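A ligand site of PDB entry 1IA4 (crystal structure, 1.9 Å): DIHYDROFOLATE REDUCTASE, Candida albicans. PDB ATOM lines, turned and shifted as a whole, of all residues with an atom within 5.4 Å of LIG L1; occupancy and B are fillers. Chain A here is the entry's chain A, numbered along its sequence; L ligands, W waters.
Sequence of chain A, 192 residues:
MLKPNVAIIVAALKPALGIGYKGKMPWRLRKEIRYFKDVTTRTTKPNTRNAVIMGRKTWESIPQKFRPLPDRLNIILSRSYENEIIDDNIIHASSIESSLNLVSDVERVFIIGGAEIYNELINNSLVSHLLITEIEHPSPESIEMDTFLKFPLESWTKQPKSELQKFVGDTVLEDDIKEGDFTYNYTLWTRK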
ATOM      1  N   LYS A  22      -0.526 -14.957  12.745  1.00  0.00           N
ATOM      2  CA  LYS A  22      -1.073 -14.358  13.991  1.00  0.00           C
ATOM      3  C   LYS A  22      -2.567 -14.387  14.052  1.00  0.00           C
ATOM      4  O   LYS A  22      -3.251 -13.389  14.396  1.00  0.00           O
ATOM      5  CB  LYS A  22      -0.488 -12.899  14.089  1.00  0.00           C
ATOM      6  N   GLY A  23      -3.133 -15.552  13.657  1.00  0.00           N
ATOM      7  CA  GLY A  23      -4.578 -15.747  13.735  1.00  0.00           C
ATOM      8  C   GLY A  23      -5.422 -15.353  12.571  1.00  0.00           C
ATOM      9  O   GLY A  23      -6.686 -15.514  12.663  1.00  0.00           O
ATOM     10  N   MET A  54     -15.065 -26.819  14.015  1.00  0.00           N
ATOM     11  CA  MET A  54     -13.985 -25.848  14.175  1.00  0.00           C
ATOM     12  C   MET A  54     -13.405 -25.897  15.601  1.00  0.00           C
ATOM     13  O   MET A  54     -14.167 -26.378  16.435  1.00  0.00           O
ATOM     14  CB  MET A  54     -14.427 -24.437  13.866  1.00  0.00           C
ATOM     15  CG  MET A  54     -15.405 -23.809  14.800  1.00  0.00           C
ATOM     16  SD  MET A  54     -16.192 -22.403  14.015  1.00  0.00           S
ATOM     17  CE  MET A  54     -17.497 -23.234  13.149  1.00  0.00           C
ATOM     18  N   GLY A  55     -12.238 -25.473  15.849  1.00  0.00           N
ATOM     19  CA  GLY A  55     -11.601 -25.398  17.156  1.00  0.00           C
ATOM     20  C   GLY A  55     -12.210 -24.199  17.848  1.00  0.00           C
ATOM     21  O   GLY A  55     -12.794 -23.286  17.216  1.00  0.00           O
ATOM     22  N   ARG A  56     -12.065 -24.198  19.169  1.00  0.00           N
ATOM     23  CA  ARG A  56     -12.667 -23.117  19.978  1.00  0.00           C
ATOM     24  C   ARG A  56     -12.045 -21.789  19.585  1.00  0.00           C
ATOM     25  O   ARG A  56     -12.790 -20.796  19.599  1.00  0.00           O
ATOM     26  CB  ARG A  56     -12.273 -23.349  21.457  1.00  0.00           C
ATOM     27  CG  ARG A  56     -13.124 -22.368  22.382  1.00  0.00           C
ATOM     28  CD  ARG A  56     -12.690 -22.474  23.789  1.00  0.00           C
ATOM     29  NE  ARG A  56     -11.286 -22.441  24.015  1.00  0.00           N
ATOM     30  CZ  ARG A  56     -10.333 -21.610  24.108  1.00  0.00           C
ATOM     31  NH1 ARG A  56      -9.062 -22.016  24.261  1.00  0.00           N
ATOM     32  NH2 ARG A  56     -10.519 -20.290  24.117  1.00  0.00           N
ATOM     33  N   LYS A  57     -10.783 -21.691  19.297  1.00  0.00           N
ATOM     34  CA  LYS A  57     -10.175 -20.374  18.945  1.00  0.00           C
ATOM     35  C   LYS A  57     -10.721 -19.773  17.675  1.00  0.00           C
ATOM     36  O   LYS A  57     -10.962 -18.552  17.588  1.00  0.00           O
ATOM     37  CB  LYS A  57      -8.659 -20.512  18.893  1.00  0.00           C
ATOM     38  CG  LYS A  57      -8.127 -20.777  20.341  1.00  0.00           C
ATOM     39  CD  LYS A  57      -6.679 -21.070  20.300  1.00  0.00           C
ATOM     40  CE  LYS A  57      -6.044 -21.643  21.543  1.00  0.00           C
ATOM     41  NZ  LYS A  57      -4.650 -22.109  21.203  1.00  0.00           N
ATOM     42  N   THR A  58     -10.953 -20.617  16.649  1.00  0.00           N
ATOM     43  CA  THR A  58     -11.575 -20.102  15.395  1.00  0.00           C
ATOM     44  C   THR A  58     -12.976 -19.602  15.732  1.00  0.00           C
ATOM     45  O   THR A  58     -13.329 -18.517  15.302  1.00  0.00           O
ATOM     46  CB  THR A  58     -11.627 -21.234  14.306  1.00  0.00           C
ATOM     47  OG1 THR A  58     -10.248 -21.607  14.042  1.00  0.00           O
ATOM     48  CG2 THR A  58     -12.415 -20.889  13.075  1.00  0.00           C
ATOM     49  N   TRP A  59     -13.784 -20.361  16.494  1.00  0.00           N
ATOM     50  CA  TRP A  59     -15.140 -19.908  16.858  1.00  0.00           C
ATOM     51  C   TRP A  59     -15.083 -18.494  17.450  1.00  0.00           C
ATOM     52  O   TRP A  59     -15.861 -17.593  17.105  1.00  0.00           O
ATOM     53  CB  TRP A  59     -15.765 -20.904  17.828  1.00  0.00           C
ATOM     54  CG  TRP A  59     -17.103 -20.497  18.394  1.00  0.00           C
ATOM     55  CD1 TRP A  59     -17.316 -19.931  19.616  1.00  0.00           C
ATOM     56  CD2 TRP A  59     -18.366 -20.554  17.763  1.00  0.00           C
ATOM     57  NE1 TRP A  59     -18.659 -19.712  19.814  1.00  0.00           N
ATOM     58  CE2 TRP A  59     -19.333 -20.073  18.683  1.00  0.00           C
ATOM     59  CE3 TRP A  59     -18.814 -21.005  16.504  1.00  0.00           C
ATOM     60  CZ2 TRP A  59     -20.657 -20.033  18.376  1.00  0.00           C
ATOM     61  CZ3 TRP A  59     -20.140 -21.025  16.244  1.00  0.00           C
ATOM     62  CH2 TRP A  59     -21.108 -20.540  17.155  1.00  0.00           C
ATOM     63  N   LEU A  77     -15.082 -27.687  19.060  1.00  0.00           N
ATOM     64  CA  LEU A  77     -14.297 -28.586  19.878  1.00  0.00           C
ATOM     65  C   LEU A  77     -13.456 -27.809  20.893  1.00  0.00           C
ATOM     66  O   LEU A  77     -12.707 -26.865  20.492  1.00  0.00           O
ATOM     67  CB  LEU A  77     -13.438 -29.511  19.018  1.00  0.00           C
ATOM     68  CG  LEU A  77     -14.090 -30.311  17.904  1.00  0.00           C
ATOM     69  CD1 LEU A  77     -13.009 -31.145  17.179  1.00  0.00           C
ATOM     70  CD2 LEU A  77     -15.098 -31.318  18.465  1.00  0.00           C
ATOM     71  N   SER A  78     -13.502 -28.310  22.110  1.00  0.00           N
ATOM     72  CA  SER A  78     -12.633 -27.736  23.170  1.00  0.00           C
ATOM     73  C   SER A  78     -12.339 -28.960  24.103  1.00  0.00           C
ATOM     74  O   SER A  78     -13.223 -29.804  24.204  1.00  0.00           O
ATOM     75  CB  SER A  78     -13.248 -26.631  24.006  1.00  0.00           C
ATOM     76  OG  SER A  78     -12.293 -26.352  25.077  1.00  0.00           O
ATOM     77  N   ARG A  79     -11.136 -29.036  24.607  1.00  0.00           N
ATOM     78  CA  ARG A  79     -10.764 -30.118  25.543  1.00  0.00           C
ATOM     79  C   ARG A  79     -11.500 -29.963  26.857  1.00  0.00           C
ATOM     80  O   ARG A  79     -11.633 -30.958  27.611  1.00  0.00           O
ATOM     81  CB  ARG A  79      -9.241 -30.194  25.732  1.00  0.00           C
ATOM     82  CG  ARG A  79      -8.614 -30.869  24.550  1.00  0.00           C
ATOM     83  CD  ARG A  79      -7.130 -30.919  24.665  1.00  0.00           C
ATOM     84  NE  ARG A  79      -6.416 -30.986  23.390  1.00  0.00           N
ATOM     85  CZ  ARG A  79      -6.000 -29.931  22.691  1.00  0.00           C
ATOM     86  NH1 ARG A  79      -6.158 -28.673  23.134  1.00  0.00           N
ATOM     87  NH2 ARG A  79      -5.394 -30.112  21.512  1.00  0.00           N
ATOM     88  N   SER A  80     -11.974 -28.753  27.140  1.00  0.00           N
ATOM     89  CA  SER A  80     -12.739 -28.414  28.342  1.00  0.00           C
ATOM     90  C   SER A  80     -14.245 -28.590  28.206  1.00  0.00           C
ATOM     91  O   SER A  80     -15.025 -28.308  29.170  1.00  0.00           O
ATOM     92  CB  SER A  80     -12.475 -27.002  28.822  1.00  0.00           C
ATOM     93  OG  SER A  80     -11.231 -26.737  29.330  1.00  0.00           O
ATOM     94  N   SER A  94     -15.884 -32.499  22.990  1.00  0.00           N
ATOM     95  CA  SER A  94     -14.461 -32.591  23.282  1.00  0.00           C
ATOM     96  C   SER A  94     -13.762 -33.532  22.313  1.00  0.00           C
ATOM     97  O   SER A  94     -12.554 -33.652  22.494  1.00  0.00           O
ATOM     98  CB  SER A  94     -14.091 -32.980  24.733  1.00  0.00           C
ATOM     99  OG  SER A  94     -14.659 -34.284  24.893  1.00  0.00           O
ATOM    100  N   SER A  95     -14.466 -34.148  21.364  1.00  0.00           N
ATOM    101  CA  SER A  95     -13.813 -35.006  20.376  1.00  0.00           C
ATOM    102  C   SER A  95     -14.725 -35.023  19.115  1.00  0.00           C
ATOM    103  O   SER A  95     -15.955 -34.815  19.250  1.00  0.00           O
ATOM    104  CB  SER A  95     -13.423 -36.422  20.744  1.00  0.00           C
ATOM    105  OG  SER A  95     -14.534 -37.268  20.945  1.00  0.00           O
ATOM    106  N   GLY A 113     -11.154 -25.703  10.495  1.00  0.00           N
ATOM    107  CA  GLY A 113      -9.974 -24.981  11.012  1.00  0.00           C
ATOM    108  C   GLY A 113     -10.069 -24.977  12.575  1.00  0.00           C
ATOM    109  O   GLY A 113     -11.114 -25.463  13.029  1.00  0.00           O
ATOM    110  N   GLY A 114      -9.113 -24.412  13.254  1.00  0.00           N
ATOM    111  CA  GLY A 114      -7.913 -23.790  12.702  1.00  0.00           C
ATOM    112  C   GLY A 114      -6.735 -24.691  12.562  1.00  0.00           C
ATOM    113  O   GLY A 114      -6.887 -25.898  12.394  1.00  0.00           O
ATOM    114  N   ALA A 115      -5.529 -24.095  12.673  1.00  0.00           N
ATOM    115  CA  ALA A 115      -4.272 -24.786  12.507  1.00  0.00           C
ATOM    116  C   ALA A 115      -4.109 -26.032  13.381  1.00  0.00           C
ATOM    117  O   ALA A 115      -3.697 -27.080  12.837  1.00  0.00           O
ATOM    118  CB  ALA A 115      -3.119 -23.878  12.820  1.00  0.00           C
ATOM    119  N   GLU A 116      -4.372 -25.844  14.659  1.00  0.00           N
ATOM    120  CA  GLU A 116      -4.201 -27.032  15.565  1.00  0.00           C
ATOM    121  C   GLU A 116      -5.204 -28.087  15.191  1.00  0.00           C
ATOM    122  O   GLU A 116      -4.800 -29.263  15.082  1.00  0.00           O
ATOM    123  CB  GLU A 116      -4.308 -26.625  17.033  1.00  0.00           C
ATOM    124  CG  GLU A 116      -4.038 -27.835  17.975  1.00  0.00           C
ATOM    125  CD  GLU A 116      -4.037 -27.560  19.440  1.00  0.00           C
ATOM    126  OE1 GLU A 116      -3.819 -28.449  20.267  1.00  0.00           O
ATOM    127  OE2 GLU A 116      -4.273 -26.397  19.813  1.00  0.00           O
ATOM    128  N   ILE A 117      -6.432 -27.724  14.872  1.00  0.00           N
ATOM    129  CA  ILE A 117      -7.437 -28.727  14.423  1.00  0.00           C
ATOM    130  C   ILE A 117      -7.001 -29.488  13.210  1.00  0.00           C
ATOM    131  O   ILE A 117      -7.097 -30.717  13.059  1.00  0.00           O
ATOM    132  CB  ILE A 117      -8.825 -27.984  14.274  1.00  0.00           C
ATOM    133  CG1 ILE A 117      -9.325 -27.551  15.653  1.00  0.00           C
ATOM    134  CG2 ILE A 117      -9.872 -28.807  13.470  1.00  0.00           C
ATOM    135  CD1 ILE A 117      -9.880 -28.670  16.606  1.00  0.00           C
ATOM    136  N   GLU A 120      -3.973 -31.919  13.853  1.00  0.00           N
ATOM    137  CA  GLU A 120      -4.310 -33.091  14.699  1.00  0.00           C
ATOM    138  C   GLU A 120      -5.239 -34.038  13.998  1.00  0.00           C
ATOM    139  O   GLU A 120      -5.051 -35.284  14.077  1.00  0.00           O
ATOM    140  CB  GLU A 120      -5.021 -32.603  15.955  1.00  0.00           C
ATOM    141  CG  GLU A 120      -4.909 -33.121  17.322  1.00  0.00           C
ATOM    142  CD  GLU A 120      -3.831 -32.476  18.173  1.00  0.00           C
ATOM    143  OE1 GLU A 120      -4.116 -31.882  19.175  1.00  0.00           O
ATOM    144  OE2 GLU A 120      -2.679 -32.680  17.714  1.00  0.00           O
ATOM    145  N   LEU A 121      -6.282 -33.571  13.330  1.00  0.00           N
ATOM    146  CA  LEU A 121      -7.316 -34.346  12.678  1.00  0.00           C
ATOM    147  C   LEU A 121      -6.982 -34.953  11.331  1.00  0.00           C
ATOM    148  O   LEU A 121      -7.588 -35.967  10.933  1.00  0.00           O
ATOM    149  CB  LEU A 121      -8.629 -33.623  12.810  1.00  0.00           C
ATOM    150  CG  LEU A 121      -9.060 -33.254  14.240  1.00  0.00           C
ATOM    151  CD1 LEU A 121     -10.234 -32.310  14.207  1.00  0.00           C
ATOM    152  CD2 LEU A 121      -9.414 -34.533  15.004  1.00  0.00           C
HETATM  153  P1  LIG L   1      -8.020 -23.653  16.444  1.00  0.00           P
HETATM  154  O1  LIG L   1      -7.447 -24.825  15.805  1.00  0.00           O
HETATM  155  O2  LIG L   1      -9.242 -23.102  15.816  1.00  0.00           O
HETATM  156  O3  LIG L   1      -8.430 -24.027  17.996  1.00  0.00           O
HETATM  157  C1  LIG L   1      -7.496 -24.776  18.803  1.00  0.00           C
HETATM  158  C2  LIG L   1      -8.327 -25.170  20.048  1.00  0.00           C
HETATM  159  O4  LIG L   1      -9.194 -26.217  19.643  1.00  0.00           O
HETATM  160  C3  LIG L   1      -7.422 -25.862  21.132  1.00  0.00           C
HETATM  161  O5  LIG L   1      -6.775 -24.773  21.776  1.00  0.00           O
HETATM  162  C4  LIG L   1      -8.571 -26.616  21.904  1.00  0.00           C
HETATM  163  O6  LIG L   1      -9.551 -25.807  22.584  1.00  0.00           O
HETATM  164  C5  LIG L   1      -9.388 -27.115  20.721  1.00  0.00           C
HETATM  165  N1  LIG L   1      -8.901 -28.351  20.260  1.00  0.00           N
HETATM  166  C6  LIG L   1      -7.780 -28.394  19.469  1.00  0.00           C
HETATM  167  N2  LIG L   1      -7.460 -29.617  19.146  1.00  0.00           N
HETATM  168  C7  LIG L   1      -8.452 -30.369  19.734  1.00  0.00           C
HETATM  169  C8  LIG L   1      -8.591 -31.763  19.736  1.00  0.00           C
HETATM  170  N3  LIG L   1      -7.717 -32.548  19.057  1.00  0.00           N
HETATM  171  N4  LIG L   1      -9.676 -32.230  20.399  1.00  0.00           N
HETATM  172  C9  LIG L   1     -10.437 -31.334  21.119  1.00  0.00           C
HETATM  173  N5  LIG L   1     -10.345 -30.037  21.194  1.00  0.00           N
HETATM  174  C10 LIG L   1      -9.330 -29.601  20.427  1.00  0.00           C
HETATM  175  O7  LIG L   1      -7.002 -22.536  16.645  1.00  0.00           O
HETATM  176  P2  LIG L   1      -5.528 -22.134  16.048  1.00  0.00           P
HETATM  177  O8  LIG L   1      -5.770 -21.745  14.621  1.00  0.00           O
HETATM  178  O9  LIG L   1      -4.628 -23.267  16.195  1.00  0.00           O
HETATM  179  O10 LIG L   1      -5.152 -20.858  16.879  1.00  0.00           O
HETATM  180  C11 LIG L   1      -4.332 -19.767  16.427  1.00  0.00           C
HETATM  181  C12 LIG L   1      -3.758 -18.912  17.545  1.00  0.00           C
HETATM  182  O11 LIG L   1      -2.316 -18.792  17.379  1.00  0.00           O
HETATM  183  C13 LIG L   1      -4.323 -17.507  17.727  1.00  0.00           C
HETATM  184  P3  LIG L   1      -9.237 -25.633  24.251  1.00  0.00           P
HETATM  185  O12 LIG L   1     -10.465 -24.788  24.524  1.00  0.00           O
HETATM  186  O13 LIG L   1      -9.078 -27.017  24.599  1.00  0.00           O
HETATM  187  O14 LIG L   1      -8.019 -24.813  24.268  1.00  0.00           O
HETATM  188  C1  LG2 L   2     -11.548 -22.683   4.783  1.00  0.00           C
HETATM  189  N1  LG2 L   2     -11.173 -23.275   3.671  1.00  0.00           N
HETATM  190  C2  LG2 L   2     -11.203 -22.631   2.494  1.00  0.00           C
HETATM  191  N2  LG2 L   2     -11.463 -21.294   2.415  1.00  0.00           N
HETATM  192  C3  LG2 L   2     -12.698 -19.152   5.853  1.00  0.00           C
HETATM  193  C4  LG2 L   2     -12.351 -20.498   5.953  1.00  0.00           C
HETATM  194  C5  LG2 L   2     -11.965 -21.276   4.850  1.00  0.00           C
HETATM  195  C6  LG2 L   2     -11.870 -20.564   3.620  1.00  0.00           C
HETATM  196  C7  LG2 L   2     -12.270 -19.242   3.511  1.00  0.00           C
HETATM  197  C8  LG2 L   2     -12.649 -18.497   4.617  1.00  0.00           C
HETATM  198  N3  LG2 L   2     -10.821 -23.257   1.384  1.00  0.00           N
HETATM  199  N4  LG2 L   2     -11.501 -23.575   5.762  1.00  0.00           N
HETATM  200  S1  LG2 L   2     -12.556 -21.193   7.583  1.00  0.00           S
HETATM  201  C9  LG2 L   2     -10.904 -20.928   8.215  1.00  0.00           C
HETATM  202  C10 LG2 L   2      -9.741 -20.768   7.465  1.00  0.00           C
HETATM  203  C11 LG2 L   2      -8.490 -20.575   8.001  1.00  0.00           C
HETATM  204  C12 LG2 L   2      -8.281 -20.585   9.437  1.00  0.00           C
HETATM  205  C13 LG2 L   2      -9.420 -20.782  10.176  1.00  0.00           C
HETATM  206  C14 LG2 L   2     -10.692 -20.910   9.620  1.00  0.00           C
HETATM  207  C15 LG2 L   2      -5.113 -20.674  11.482  1.00  0.00           C
HETATM  208  C16 LG2 L   2      -5.956 -21.053  10.311  1.00  0.00           C
HETATM  209  N5  LG2 L   2      -7.084 -20.270   9.943  1.00  0.00           N
HETATM  210  C17 LG2 L   2      -7.015 -18.791  10.385  1.00  0.00           C
HETATM  211  C18 LG2 L   2      -5.557 -18.528  10.770  1.00  0.00           C
HETATM  212  O1  LG2 L   2      -5.347 -19.361  11.928  1.00  0.00           O
HETATM  213  O   HOH W   1     -10.219 -23.916  26.957  1.00  0.00           O
HETATM  214  O   HOH W   2      -6.698 -27.485  25.366  1.00  0.00           O
HETATM  215  O   HOH W   3      -4.052 -23.593  18.973  1.00  0.00           O
HETATM  216  O   HOH W   4      -5.826 -33.278  21.455  1.00  0.00           O
HETATM  217  O   HOH W   5      -4.339 -25.277  22.183  1.00  0.00           O
HETATM  218  O   HOH W   6      -7.383 -35.482  20.177  1.00  0.00           O
HETATM  219  O   HOH W   7      -1.733 -23.744  16.082  1.00  0.00           O
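Merely in contact with LIG L1: Gly 55, Leu 77, Ser 94, Gly 113 and Glu 120.
Hydrophobic or aromatic side chains within 4 Å of LIG L1: Leu 77, Ala 115 and Ile 117.
Of the 21 residues printed, 14 come within 4 Å of LIG L1.
The nearest printed residue that does not touch LIG L1 is Ser 80 (4.2 Å).
Water W5 lies within hydrogen-bond range of O5 of LIG L1 (2.5 Å), OE2 of Glu 116 (2.6 Å) and NZ of Lys 57 (3.3 Å).
Water W2 lies within hydrogen-bond range of an oxygen (O13) of LIG L1 (2.5 Å) and the guanidinium group (NH1) of Arg 79 (2.6 Å).
Water W1 lies within hydrogen-bond range of O12 of LIG L1 (2.6 Å) and NE of Arg 56 (3.5 Å).
Water W3 lies within hydrogen-bond range of the side-chain amino group of Lys 57, an oxygen (O9) of LIG L1 and the side-chain carboxylate of Glu 116.
Water W4 lies within hydrogen-bond range of the guanidinium group of Arg 79 (3.1 Å), a nitrogen (N3) of LIG L1 (3.1 Å) and the side-chain carboxylate of Glu 120 (3.2 Å).
The side-chain hydroxyl of Ser 78 sits close to the backbone NH of Ser 80, at 3.2 Å.
NH2 of Arg 79 is in salt-bridge range of OE1 of Glu 116, at 2.6 Å.
N of Gly 55 lies within hydrogen-bond range of O of Gly 113.
The backbone NH (N) of Arg 56 is in hydrogen-bond range of the backbone carbonyl oxygen (O) of Leu 77.
N of Gly 114 lies within hydrogen-bond range of OG1 of Thr 58.
The side-chain carboxylate (OE1) of Glu 120 lies within salt-bridge range of the guanidinium group (NH2) of Arg 79 (3.2 Å).
The backbone NH of Leu 77 is in hydrogen-bond range of the backbone carbonyl oxygen of Met 54, at 3.1 Å.
The guanidinium group (NH1) of Arg 79 is in salt-bridge range of an oxygen (O13) of LIG L1.
The side-chain amino group of Lys 57 sits close to an oxygen (O5) of LIG L1 (3.5 Å).
An oxygen (O2) of LIG L1 is in hydrogen-bond range of the backbone NH (N) of Thr 58.
The guanidinium group of Arg 56 lies within salt-bridge range of an oxygen (O12) of LIG L1 (2.5 Å).
OG of Ser 78 lies within hydrogen-bond range of O12 of LIG L1 (2.5 Å).
The backbone NH (N) of Arg 79 is in hydrogen-bond range of an oxygen (O13) of LIG L1, at 2.9 Å.
The backbone NH (N) of Glu 116 is in hydrogen-bond range of an oxygen (O9) of LIG L1, 3.0 Å away.
The backbone NH (N) of Gly 114 lies within hydrogen-bond range of an oxygen (O2) of LIG L1, at 2.9 Å.
O2 of LIG L1 is in hydrogen-bond range of OG1 of Thr 58 (2.5 Å).
The backbone NH (N) of Ala 115 sits at hydrogen-bond distance from an oxygen (O8) of LIG L1, at 3.1 Å.
N of Ile 117 is in hydrogen-bond range of O1 of LIG L1 (3.2 Å).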
